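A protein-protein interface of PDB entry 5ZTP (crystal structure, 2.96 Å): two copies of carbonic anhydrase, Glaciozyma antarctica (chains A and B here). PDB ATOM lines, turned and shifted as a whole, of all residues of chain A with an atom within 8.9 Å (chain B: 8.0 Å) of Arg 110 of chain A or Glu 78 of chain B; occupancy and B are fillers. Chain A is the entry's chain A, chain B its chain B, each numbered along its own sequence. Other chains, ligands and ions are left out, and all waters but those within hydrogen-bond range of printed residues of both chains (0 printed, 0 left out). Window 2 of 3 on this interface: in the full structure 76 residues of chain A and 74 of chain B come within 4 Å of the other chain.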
ATOM      1  N   MET A  39       7.897  32.732 -19.859  1.00  0.00           N
ATOM      2  CA  MET A  39       7.260  32.570 -18.539  1.00  0.00           C
ATOM      3  C   MET A  39       8.235  32.371 -17.375  1.00  0.00           C
ATOM      4  O   MET A  39       7.800  32.106 -16.259  1.00  0.00           O
ATOM      5  CB  MET A  39       6.326  31.348 -18.563  1.00  0.00           C
ATOM      6  CG  MET A  39       7.057  29.989 -18.631  1.00  0.00           C
ATOM      7  SD  MET A  39       6.023  28.522 -18.492  1.00  0.00           S
ATOM      8  CE  MET A  39       7.177  27.209 -18.865  1.00  0.00           C
ATOM      9  N   PHE A  98      15.478  20.990 -24.350  1.00  0.00           N
ATOM     10  CA  PHE A  98      14.804  19.807 -24.896  1.00  0.00           C
ATOM     11  C   PHE A  98      14.202  19.938 -26.305  1.00  0.00           C
ATOM     12  O   PHE A  98      14.188  21.010 -26.927  1.00  0.00           O
ATOM     13  CB  PHE A  98      13.709  19.349 -23.925  1.00  0.00           C
ATOM     14  CG  PHE A  98      12.456  20.168 -24.009  1.00  0.00           C
ATOM     15  CD1 PHE A  98      12.392  21.428 -23.435  1.00  0.00           C
ATOM     16  CD2 PHE A  98      11.336  19.694 -24.682  1.00  0.00           C
ATOM     17  CE1 PHE A  98      11.235  22.194 -23.513  1.00  0.00           C
ATOM     18  CE2 PHE A  98      10.170  20.466 -24.759  1.00  0.00           C
ATOM     19  CZ  PHE A  98      10.129  21.724 -24.177  1.00  0.00           C
ATOM     20  N   GLN A 102      11.254  14.407 -27.257  1.00  0.00           N
ATOM     21  CA  GLN A 102      11.760  14.004 -25.931  1.00  0.00           C
ATOM     22  C   GLN A 102      10.707  14.245 -24.878  1.00  0.00           C
ATOM     23  O   GLN A 102      10.464  13.373 -24.024  1.00  0.00           O
ATOM     24  CB  GLN A 102      13.009  14.764 -25.510  1.00  0.00           C
ATOM     25  CG  GLN A 102      14.141  14.774 -26.515  1.00  0.00           C
ATOM     26  CD  GLN A 102      15.315  15.579 -26.014  1.00  0.00           C
ATOM     27  OE1 GLN A 102      15.187  16.762 -25.667  1.00  0.00           O
ATOM     28  NE2 GLN A 102      16.467  14.947 -25.963  1.00  0.00           N
ATOM     29  N   LEU A 103      10.076  15.424 -24.944  1.00  0.00           N
ATOM     30  CA  LEU A 103       9.021  15.756 -24.010  1.00  0.00           C
ATOM     31  C   LEU A 103       7.816  14.830 -24.166  1.00  0.00           C
ATOM     32  O   LEU A 103       7.248  14.383 -23.160  1.00  0.00           O
ATOM     33  CB  LEU A 103       8.560  17.201 -24.162  1.00  0.00           C
ATOM     34  CG  LEU A 103       7.364  17.525 -23.221  1.00  0.00           C
ATOM     35  CD1 LEU A 103       7.649  18.783 -22.431  1.00  0.00           C
ATOM     36  CD2 LEU A 103       6.011  17.643 -23.928  1.00  0.00           C
ATOM     37  N   HIS A 104       7.426  14.566 -25.411  1.00  0.00           N
ATOM     38  CA  HIS A 104       6.335  13.645 -25.678  1.00  0.00           C
ATOM     39  C   HIS A 104       6.537  12.318 -24.960  1.00  0.00           C
ATOM     40  O   HIS A 104       5.666  11.881 -24.198  1.00  0.00           O
ATOM     41  CB  HIS A 104       6.196  13.385 -27.178  1.00  0.00           C
ATOM     42  CG  HIS A 104       5.654  14.543 -27.928  1.00  0.00           C
ATOM     43  ND1 HIS A 104       5.650  14.597 -29.296  1.00  0.00           N
ATOM     44  CD2 HIS A 104       5.142  15.719 -27.496  1.00  0.00           C
ATOM     45  CE1 HIS A 104       5.138  15.756 -29.679  1.00  0.00           C
ATOM     46  NE2 HIS A 104       4.825  16.455 -28.604  1.00  0.00           N
ATOM     47  N   GLY A 105       7.696  11.697 -25.212  1.00  0.00           N
ATOM     48  CA  GLY A 105       8.055  10.399 -24.633  1.00  0.00           C
ATOM     49  C   GLY A 105       8.101  10.401 -23.115  1.00  0.00           C
ATOM     50  O   GLY A 105       7.936   9.346 -22.470  1.00  0.00           O
ATOM     51  N   LEU A 106       8.325  11.588 -22.547  1.00  0.00           N
ATOM     52  CA  LEU A 106       8.387  11.767 -21.098  1.00  0.00           C
ATOM     53  C   LEU A 106       7.009  11.719 -20.497  1.00  0.00           C
ATOM     54  O   LEU A 106       6.714  10.881 -19.658  1.00  0.00           O
ATOM     55  CB  LEU A 106       9.004  13.119 -20.788  1.00  0.00           C
ATOM     56  CG  LEU A 106       9.523  13.351 -19.393  1.00  0.00           C
ATOM     57  CD1 LEU A 106      10.655  12.396 -19.097  1.00  0.00           C
ATOM     58  CD2 LEU A 106      10.039  14.776 -19.339  1.00  0.00           C
ATOM     59  N   VAL A 107       6.162  12.617 -20.974  1.00  0.00           N
ATOM     60  CA  VAL A 107       4.817  12.725 -20.497  1.00  0.00           C
ATOM     61  C   VAL A 107       4.100  11.407 -20.742  1.00  0.00           C
ATOM     62  O   VAL A 107       3.210  11.026 -19.969  1.00  0.00           O
ATOM     63  CB  VAL A 107       4.100  13.886 -21.205  1.00  0.00           C
ATOM     64  CG1 VAL A 107       2.618  13.942 -20.843  1.00  0.00           C
ATOM     65  CG2 VAL A 107       4.784  15.185 -20.830  1.00  0.00           C
ATOM     66  N   LYS A 108       4.492  10.717 -21.820  1.00  0.00           N
ATOM     67  CA  LYS A 108       3.971   9.363 -22.136  1.00  0.00           C
ATOM     68  C   LYS A 108       4.224   8.344 -21.027  1.00  0.00           C
ATOM     69  O   LYS A 108       3.398   7.471 -20.769  1.00  0.00           O
ATOM     70  CB  LYS A 108       4.569   8.829 -23.442  1.00  0.00           C
ATOM     71  CG  LYS A 108       3.783   9.231 -24.674  1.00  0.00           C
ATOM     72  CD  LYS A 108       4.360   8.575 -25.897  1.00  0.00           C
ATOM     73  CE  LYS A 108       3.969   9.307 -27.153  1.00  0.00           C
ATOM     74  NZ  LYS A 108       3.838   8.310 -28.255  1.00  0.00           N
ATOM     75  N   LYS A 109       5.367   8.497 -20.372  1.00  0.00           N
ATOM     76  CA  LYS A 109       5.768   7.614 -19.292  1.00  0.00           C
ATOM     77  C   LYS A 109       4.980   7.841 -17.990  1.00  0.00           C
ATOM     78  O   LYS A 109       5.085   7.018 -17.083  1.00  0.00           O
ATOM     79  CB  LYS A 109       7.289   7.731 -19.038  1.00  0.00           C
ATOM     80  CG  LYS A 109       8.206   7.147 -20.132  1.00  0.00           C
ATOM     81  CD  LYS A 109       9.181   6.131 -19.564  1.00  0.00           C
ATOM     82  CE  LYS A 109       9.281   4.868 -20.393  1.00  0.00           C
ATOM     83  NZ  LYS A 109       8.155   3.902 -20.125  1.00  0.00           N
ATOM     84  N   ARG A 110       4.170   8.912 -17.934  1.00  0.00           N
ATOM     85  CA  ARG A 110       3.442   9.363 -16.716  1.00  0.00           C
ATOM     86  C   ARG A 110       1.925   9.455 -16.876  1.00  0.00           C
ATOM     87  O   ARG A 110       1.259  10.073 -16.057  1.00  0.00           O
ATOM     88  CB  ARG A 110       3.934  10.761 -16.303  1.00  0.00           C
ATOM     89  CG  ARG A 110       5.442  10.914 -16.348  1.00  0.00           C
ATOM     90  CD  ARG A 110       5.881  12.309 -15.945  1.00  0.00           C
ATOM     91  NE  ARG A 110       7.340  12.399 -15.791  1.00  0.00           N
ATOM     92  CZ  ARG A 110       8.054  13.526 -15.886  1.00  0.00           C
ATOM     93  NH1 ARG A 110       7.465  14.697 -16.154  1.00  0.00           N
ATOM     94  NH2 ARG A 110       9.379  13.486 -15.735  1.00  0.00           N
ATOM     95  N   VAL A 111       1.385   8.901 -17.955  1.00  0.00           N
ATOM     96  CA  VAL A 111      -0.032   9.027 -18.263  1.00  0.00           C
ATOM     97  C   VAL A 111      -0.438   7.791 -19.043  1.00  0.00           C
ATOM     98  O   VAL A 111       0.399   7.202 -19.724  1.00  0.00           O
ATOM     99  CB  VAL A 111      -0.348  10.276 -19.140  1.00  0.00           C
ATOM    100  CG1 VAL A 111       0.018  11.574 -18.440  1.00  0.00           C
ATOM    101  CG2 VAL A 111       0.346  10.212 -20.491  1.00  0.00           C
ATOM    102  N   ALA A 112      -1.723   7.430 -18.952  1.00  0.00           N
ATOM    103  CA  ALA A 112      -2.306   6.275 -19.650  1.00  0.00           C
ATOM    104  C   ALA A 112      -2.251   6.376 -21.185  1.00  0.00           C
ATOM    105  O   ALA A 112      -2.299   7.460 -21.751  1.00  0.00           O
ATOM    106  CB  ALA A 112      -3.738   6.076 -19.194  1.00  0.00           C
ATOM    107  N   HIS A 113      -2.176   5.218 -21.840  1.00  0.00           N
ATOM    108  CA  HIS A 113      -1.949   5.114 -23.307  1.00  0.00           C
ATOM    109  C   HIS A 113      -3.002   5.889 -24.078  1.00  0.00           C
ATOM    110  O   HIS A 113      -2.737   6.454 -25.123  1.00  0.00           O
ATOM    111  CB  HIS A 113      -1.911   3.637 -23.777  1.00  0.00           C
ATOM    112  CG  HIS A 113      -0.816   2.822 -23.140  1.00  0.00           C
ATOM    113  ND1 HIS A 113      -0.829   2.455 -21.804  1.00  0.00           N
ATOM    114  CD2 HIS A 113       0.323   2.304 -23.658  1.00  0.00           C
ATOM    115  CE1 HIS A 113       0.253   1.747 -21.530  1.00  0.00           C
ATOM    116  NE2 HIS A 113       0.970   1.643 -22.636  1.00  0.00           N
ATOM    117  N   HIS A 115      -3.991   8.690 -23.728  1.00  0.00           N
ATOM    118  CA  HIS A 115      -3.697  10.122 -23.859  1.00  0.00           C
ATOM    119  C   HIS A 115      -2.429  10.440 -24.668  1.00  0.00           C
ATOM    120  O   HIS A 115      -2.020  11.581 -24.750  1.00  0.00           O
ATOM    121  CB  HIS A 115      -3.565  10.722 -22.462  1.00  0.00           C
ATOM    122  CG  HIS A 115      -4.736  10.431 -21.571  1.00  0.00           C
ATOM    123  ND1 HIS A 115      -5.987  10.969 -21.788  1.00  0.00           N
ATOM    124  CD2 HIS A 115      -4.843   9.664 -20.461  1.00  0.00           C
ATOM    125  CE1 HIS A 115      -6.817  10.537 -20.853  1.00  0.00           C
ATOM    126  NE2 HIS A 115      -6.148   9.743 -20.038  1.00  0.00           N
ATOM    127  N   PHE A 116      -1.824   9.420 -25.257  1.00  0.00           N
ATOM    128  CA  PHE A 116      -0.595   9.563 -26.033  1.00  0.00           C
ATOM    129  C   PHE A 116      -0.844  10.450 -27.260  1.00  0.00           C
ATOM    130  O   PHE A 116      -0.055  11.354 -27.581  1.00  0.00           O
ATOM    131  CB  PHE A 116      -0.093   8.180 -26.452  1.00  0.00           C
ATOM    132  CG  PHE A 116       0.525   7.367 -25.322  1.00  0.00           C
ATOM    133  CD1 PHE A 116       0.412   7.747 -23.984  1.00  0.00           C
ATOM    134  CD2 PHE A 116       1.213   6.205 -25.602  1.00  0.00           C
ATOM    135  CE1 PHE A 116       0.994   6.996 -22.972  1.00  0.00           C
ATOM    136  CE2 PHE A 116       1.786   5.463 -24.592  1.00  0.00           C
ATOM    137  CZ  PHE A 116       1.676   5.856 -23.276  1.00  0.00           C
ATOM    138  N   VAL A 119      -0.694  14.162 -26.068  1.00  0.00           N
ATOM    139  CA  VAL A 119       0.695  14.641 -25.852  1.00  0.00           C
ATOM    140  C   VAL A 119       1.357  14.916 -27.192  1.00  0.00           C
ATOM    141  O   VAL A 119       2.032  15.924 -27.350  1.00  0.00           O
ATOM    142  CB  VAL A 119       1.608  13.728 -24.951  1.00  0.00           C
ATOM    143  CG1 VAL A 119       0.840  12.630 -24.224  1.00  0.00           C
ATOM    144  CG2 VAL A 119       2.754  13.104 -25.731  1.00  0.00           C
ATOM    145  N   LEU A 122       1.143  18.357 -29.155  1.00  0.00           N
ATOM    146  CA  LEU A 122       1.812  19.600 -28.688  1.00  0.00           C
ATOM    147  C   LEU A 122       3.111  19.942 -29.415  1.00  0.00           C
ATOM    148  O   LEU A 122       4.115  19.248 -29.256  1.00  0.00           O
ATOM    149  CB  LEU A 122       2.197  19.479 -27.215  1.00  0.00           C
ATOM    150  CG  LEU A 122       1.062  19.515 -26.204  1.00  0.00           C
ATOM    151  CD1 LEU A 122       1.702  19.299 -24.841  1.00  0.00           C
ATOM    152  CD2 LEU A 122       0.272  20.830 -26.272  1.00  0.00           C
ATOM    153  N   ARG B  71       0.052  24.299 -23.025  1.00  0.00           N
ATOM    154  CA  ARG B  71       1.359  23.894 -23.518  1.00  0.00           C
ATOM    155  C   ARG B  71       2.463  24.382 -22.562  1.00  0.00           C
ATOM    156  O   ARG B  71       3.420  23.664 -22.275  1.00  0.00           O
ATOM    157  CB  ARG B  71       1.539  24.438 -24.942  1.00  0.00           C
ATOM    158  CG  ARG B  71       2.958  24.437 -25.470  1.00  0.00           C
ATOM    159  CD  ARG B  71       3.268  25.672 -26.315  1.00  0.00           C
ATOM    160  NE  ARG B  71       4.679  25.967 -26.167  1.00  0.00           N
ATOM    161  CZ  ARG B  71       5.221  27.153 -25.898  1.00  0.00           C
ATOM    162  NH1 ARG B  71       4.510  28.273 -25.814  1.00  0.00           N
ATOM    163  NH2 ARG B  71       6.541  27.209 -25.747  1.00  0.00           N
ATOM    164  N   SER B  72       2.311  25.610 -22.074  1.00  0.00           N
ATOM    165  CA  SER B  72       3.277  26.211 -21.164  1.00  0.00           C
ATOM    166  C   SER B  72       3.251  25.447 -19.865  1.00  0.00           C
ATOM    167  O   SER B  72       4.277  25.281 -19.223  1.00  0.00           O
ATOM    168  CB  SER B  72       2.948  27.692 -20.900  1.00  0.00           C
ATOM    169  OG  SER B  72       3.249  28.503 -22.016  1.00  0.00           O
ATOM    170  N   LEU B  73       2.060  24.990 -19.490  1.00  0.00           N
ATOM    171  CA  LEU B  73       1.853  24.310 -18.212  1.00  0.00           C
ATOM    172  C   LEU B  73       2.477  22.921 -18.219  1.00  0.00           C
ATOM    173  O   LEU B  73       3.155  22.501 -17.275  1.00  0.00           O
ATOM    174  CB  LEU B  73       0.357  24.191 -17.910  1.00  0.00           C
ATOM    175  CG  LEU B  73      -0.314  25.433 -17.349  1.00  0.00           C
ATOM    176  CD1 LEU B  73      -1.799  25.183 -17.262  1.00  0.00           C
ATOM    177  CD2 LEU B  73       0.250  25.769 -15.982  1.00  0.00           C
ATOM    178  N   VAL B  74       2.280  22.223 -19.314  1.00  0.00           N
ATOM    179  CA  VAL B  74       2.882  20.943 -19.462  1.00  0.00           C
ATOM    180  C   VAL B  74       4.395  21.092 -19.321  1.00  0.00           C
ATOM    181  O   VAL B  74       5.023  20.340 -18.597  1.00  0.00           O
ATOM    182  CB  VAL B  74       2.417  20.286 -20.778  1.00  0.00           C
ATOM    183  CG1 VAL B  74       3.230  19.030 -21.113  1.00  0.00           C
ATOM    184  CG2 VAL B  74       0.923  19.952 -20.649  1.00  0.00           C
ATOM    185  N   ILE B  75       4.978  22.085 -19.958  1.00  0.00           N
ATOM    186  CA  ILE B  75       6.415  22.318 -19.813  1.00  0.00           C
ATOM    187  C   ILE B  75       6.794  22.702 -18.373  1.00  0.00           C
ATOM    188  O   ILE B  75       7.719  22.140 -17.801  1.00  0.00           O
ATOM    189  CB  ILE B  75       6.889  23.355 -20.842  1.00  0.00           C
ATOM    190  CG1 ILE B  75       6.891  22.696 -22.226  1.00  0.00           C
ATOM    191  CG2 ILE B  75       8.267  23.905 -20.497  1.00  0.00           C
ATOM    192  CD1 ILE B  75       6.766  23.662 -23.399  1.00  0.00           C
ATOM    193  N   SER B  76       6.068  23.634 -17.780  1.00  0.00           N
ATOM    194  CA  SER B  76       6.344  24.046 -16.383  1.00  0.00           C
ATOM    195  C   SER B  76       6.357  22.842 -15.426  1.00  0.00           C
ATOM    196  O   SER B  76       7.285  22.693 -14.641  1.00  0.00           O
ATOM    197  CB  SER B  76       5.344  25.125 -15.924  1.00  0.00           C
ATOM    198  OG  SER B  76       5.402  25.385 -14.548  1.00  0.00           O
ATOM    199  N   GLN B  77       5.345  21.978 -15.525  1.00  0.00           N
ATOM    200  CA  GLN B  77       5.242  20.777 -14.672  1.00  0.00           C
ATOM    201  C   GLN B  77       6.298  19.696 -14.921  1.00  0.00           C
ATOM    202  O   GLN B  77       7.046  19.326 -14.022  1.00  0.00           O
ATOM    203  CB  GLN B  77       3.875  20.121 -14.853  1.00  0.00           C
ATOM    204  CG  GLN B  77       2.701  20.923 -14.313  1.00  0.00           C
ATOM    205  CD  GLN B  77       1.485  20.055 -13.972  1.00  0.00           C
ATOM    206  OE1 GLN B  77       1.214  19.029 -14.605  1.00  0.00           O
ATOM    207  NE2 GLN B  77       0.744  20.477 -12.969  1.00  0.00           N
ATOM    208  N   GLU B  78       6.332  19.205 -16.156  1.00  0.00           N
ATOM    209  CA  GLU B  78       7.077  17.978 -16.524  1.00  0.00           C
ATOM    210  C   GLU B  78       8.593  18.226 -16.625  1.00  0.00           C
ATOM    211  O   GLU B  78       9.408  17.335 -16.437  1.00  0.00           O
ATOM    212  CB  GLU B  78       6.580  17.420 -17.877  1.00  0.00           C
ATOM    213  CG  GLU B  78       5.067  17.341 -18.051  1.00  0.00           C
ATOM    214  CD  GLU B  78       4.430  16.194 -17.288  1.00  0.00           C
ATOM    215  OE1 GLU B  78       5.022  15.109 -17.222  1.00  0.00           O
ATOM    216  OE2 GLU B  78       3.313  16.373 -16.756  1.00  0.00           O
ATOM    217  N   LEU B  79       8.939  19.456 -16.960  1.00  0.00           N
ATOM    218  CA  LEU B  79      10.319  19.850 -17.126  1.00  0.00           C
ATOM    219  C   LEU B  79      10.851  20.601 -15.908  1.00  0.00           C
ATOM    220  O   LEU B  79      12.004  20.446 -15.570  1.00  0.00           O
ATOM    221  CB  LEU B  79      10.457  20.735 -18.365  1.00  0.00           C
ATOM    222  CG  LEU B  79      11.033  20.217 -19.665  1.00  0.00           C
ATOM    223  CD1 LEU B  79      12.545  20.256 -19.482  1.00  0.00           C
ATOM    224  CD2 LEU B  79      10.542  18.834 -20.048  1.00  0.00           C
ATOM    225  N   LEU B  80      10.028  21.419 -15.257  1.00  0.00           N
ATOM    226  CA  LEU B  80      10.526  22.285 -14.197  1.00  0.00           C
ATOM    227  C   LEU B  80       9.841  22.152 -12.830  1.00  0.00           C
ATOM    228  O   LEU B  80       9.957  23.055 -12.008  1.00  0.00           O
ATOM    229  CB  LEU B  80      10.452  23.725 -14.685  1.00  0.00           C
ATOM    230  CG  LEU B  80      11.187  23.898 -16.015  1.00  0.00           C
ATOM    231  CD1 LEU B  80      10.774  25.146 -16.778  1.00  0.00           C
ATOM    232  CD2 LEU B  80      12.684  23.897 -15.760  1.00  0.00           C
ATOM    233  N   GLY B  81       9.195  21.022 -12.552  1.00  0.00           N
ATOM    234  CA  GLY B  81       8.585  20.788 -11.236  1.00  0.00           C
ATOM    235  C   GLY B  81       7.751  21.964 -10.734  1.00  0.00           C
ATOM    236  O   GLY B  81       8.272  22.987 -10.276  1.00  0.00           O
ATOM    237  N   THR B  82       6.449  21.860 -10.895  1.00  0.00           N
ATOM    238  CA  THR B  82       5.519  22.849 -10.385  1.00  0.00           C
ATOM    239  C   THR B  82       4.328  21.989 -10.146  1.00  0.00           C
ATOM    240  O   THR B  82       3.905  21.249 -11.022  1.00  0.00           O
ATOM    241  CB  THR B  82       5.133  24.009 -11.370  1.00  0.00           C
ATOM    242  OG1 THR B  82       4.146  23.583 -12.335  1.00  0.00           O
ATOM    243  CG2 THR B  82       6.330  24.605 -12.046  1.00  0.00           C
ATOM    244  N   PRO B 145      -5.888  15.368 -18.344  1.00  0.00           N
ATOM    245  CA  PRO B 145      -5.034  14.215 -18.089  1.00  0.00           C
ATOM    246  C   PRO B 145      -3.545  14.526 -18.248  1.00  0.00           C
ATOM    247  O   PRO B 145      -2.710  13.832 -17.658  1.00  0.00           O
ATOM    248  CB  PRO B 145      -5.512  13.192 -19.130  1.00  0.00           C
ATOM    249  CG  PRO B 145      -6.099  14.016 -20.229  1.00  0.00           C
ATOM    250  CD  PRO B 145      -6.747  15.163 -19.533  1.00  0.00           C
ATOM    251  N   LEU B 146      -3.221  15.528 -19.061  1.00  0.00           N
ATOM    252  CA  LEU B 146      -1.844  16.018 -19.223  1.00  0.00           C
ATOM    253  C   LEU B 146      -1.323  16.908 -18.106  1.00  0.00           C
ATOM    254  O   LEU B 146      -0.173  17.308 -18.153  1.00  0.00           O
ATOM    255  CB  LEU B 146      -1.702  16.780 -20.528  1.00  0.00           C
ATOM    256  CG  LEU B 146      -1.200  15.964 -21.700  1.00  0.00           C
ATOM    257  CD1 LEU B 146      -1.696  14.532 -21.686  1.00  0.00           C
ATOM    258  CD2 LEU B 146      -1.598  16.679 -22.976  1.00  0.00           C
ATOM    259  N   ILE B 147      -2.165  17.222 -17.127  1.00  0.00           N
ATOM    260  CA  ILE B 147      -1.748  17.892 -15.907  1.00  0.00           C
ATOM    261  C   ILE B 147      -1.585  16.805 -14.870  1.00  0.00           C
ATOM    262  O   ILE B 147      -2.369  15.867 -14.824  1.00  0.00           O
ATOM    263  CB  ILE B 147      -2.831  18.851 -15.410  1.00  0.00           C
ATOM    264  CG1 ILE B 147      -3.069  19.934 -16.435  1.00  0.00           C
ATOM    265  CG2 ILE B 147      -2.450  19.501 -14.089  1.00  0.00           C
ATOM    266  CD1 ILE B 147      -1.950  20.933 -16.509  1.00  0.00           C
ATOM    267  N   LEU B 148      -0.584  16.933 -14.011  1.00  0.00           N
ATOM    268  CA  LEU B 148      -0.308  15.879 -13.044  1.00  0.00           C
ATOM    269  C   LEU B 148      -1.411  15.752 -12.012  1.00  0.00           C
ATOM    270  O   LEU B 148      -1.967  16.740 -11.556  1.00  0.00           O
ATOM    271  CB  LEU B 148       1.003  16.132 -12.339  1.00  0.00           C
ATOM    272  CG  LEU B 148       2.216  16.210 -13.256  1.00  0.00           C
ATOM    273  CD1 LEU B 148       3.419  16.641 -12.417  1.00  0.00           C
ATOM    274  CD2 LEU B 148       2.443  14.902 -14.002  1.00  0.00           C
ATOM    275  N   PRO B 149      -1.725  14.523 -11.630  1.00  0.00           N
ATOM    276  CA  PRO B 149      -2.854  14.276 -10.719  1.00  0.00           C
ATOM    277  C   PRO B 149      -2.730  14.917  -9.293  1.00  0.00           C
ATOM    278  O   PRO B 149      -3.734  15.200  -8.624  1.00  0.00           O
ATOM    279  CB  PRO B 149      -2.886  12.744 -10.646  1.00  0.00           C
ATOM    280  CG  PRO B 149      -1.497  12.308 -11.021  1.00  0.00           C
ATOM    281  CD  PRO B 149      -1.094  13.272 -12.078  1.00  0.00           C
ATOM    282  N   GLU B 150      -1.504  15.145  -8.845  1.00  0.00           N
ATOM    283  CA  GLU B 150      -1.292  15.723  -7.527  1.00  0.00           C
ATOM    284  C   GLU B 150      -1.360  17.263  -7.531  1.00  0.00           C
ATOM    285  O   GLU B 150      -1.202  17.896  -6.495  1.00  0.00           O
ATOM    286  CB  GLU B 150       0.063  15.253  -6.979  1.00  0.00           C
ATOM    287  CG  GLU B 150       1.280  15.727  -7.787  1.00  0.00           C
ATOM    288  CD  GLU B 150       1.902  14.632  -8.644  1.00  0.00           C
ATOM    289  OE1 GLU B 150       1.155  13.953  -9.412  1.00  0.00           O
ATOM    290  OE2 GLU B 150       3.143  14.476  -8.546  1.00  0.00           O
ATOM    291  N   THR B 151      -1.588  17.880  -8.686  1.00  0.00           N
ATOM    292  CA  THR B 151      -1.482  19.338  -8.777  1.00  0.00           C
ATOM    293  C   THR B 151      -2.561  20.015  -7.945  1.00  0.00           C
ATOM    294  O   THR B 151      -3.725  19.651  -8.021  1.00  0.00           O
ATOM    295  CB  THR B 151      -1.559  19.809 -10.237  1.00  0.00           C
ATOM    296  OG1 THR B 151      -0.594  19.068 -10.982  1.00  0.00           O
ATOM    297  CG2 THR B 151      -1.270  21.310 -10.376  1.00  0.00           C
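NH1 of Arg 110 of chain A is in salt-bridge range of OE1 of Glu 78 of chain B (2.7 Å).
The backbone carbonyl oxygen (O) of Ser 72 of chain B sits close to the side-chain sulfur (SD) of Met 39 of chain A (3.8 Å).
The backbone carbonyl oxygen (O) of Ser 76 of chain B lies within hydrogen-bond range of the backbone NH (N) of Gly 81 of chain B.
OG1 of Thr 82 of chain B sits close to OG of Ser 76 of chain B, 3.1 Å away.
Among the printed residues, pairs that only touch across the chains: Met 39 of chain A with Ile 75 of chain B, Met 39 of chain A with Ser 76 of chain B, Phe 98 of chain A with Ile 75 of chain B, Leu 103 of chain A with Ile 75 of chain B, Leu 103 of chain A with Leu 79 of chain B, Leu 106 of chain A with Glu 78 of chain B, Val 107 of chain A with Glu 78 of chain B, Val 111 of chain A with Pro 145 of chain B and His 115 of chain A with Pro 145 of chain B.
Of chain B, only Glu 78 (2.7 Å) comes within 4 Å of Arg 110 of chain A.
Printed residues of chain B within 4 Å of His 115 of chain A: Pro 145.
Of the printed residues of chain A, Pro 145 of chain B touches Val 111 (3.6 Å) and His 115 (3.4 Å).
The nearest residue of chain B that does not touch Arg 110 of chain A is Leu 148 of chain B (4.7 Å).
The nearest residue of chain A that does not touch Glu 78 of chain B is Leu 103 of chain A (4.9 Å).
The nearest printed residue of chain A that does not touch Leu 79 of chain B is Phe 98 of chain A (4.1 Å).
Of the 19 printed residues of chain B, 6 touch a printed residue of chain A.
Of the 18 printed residues of chain A, 8 touch a printed residue of chain B.
Hydrophobic or aromatic side chains of chain A that line the printed part of chain B: Met 39, Phe 98, Leu 103, Leu 106, Val 107, Val 111 and His 115.
No position is printed for both chains.
Of the 11 pairs that touch across the chains among the printed residues, none has its exchanged pair printed and touching as well.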
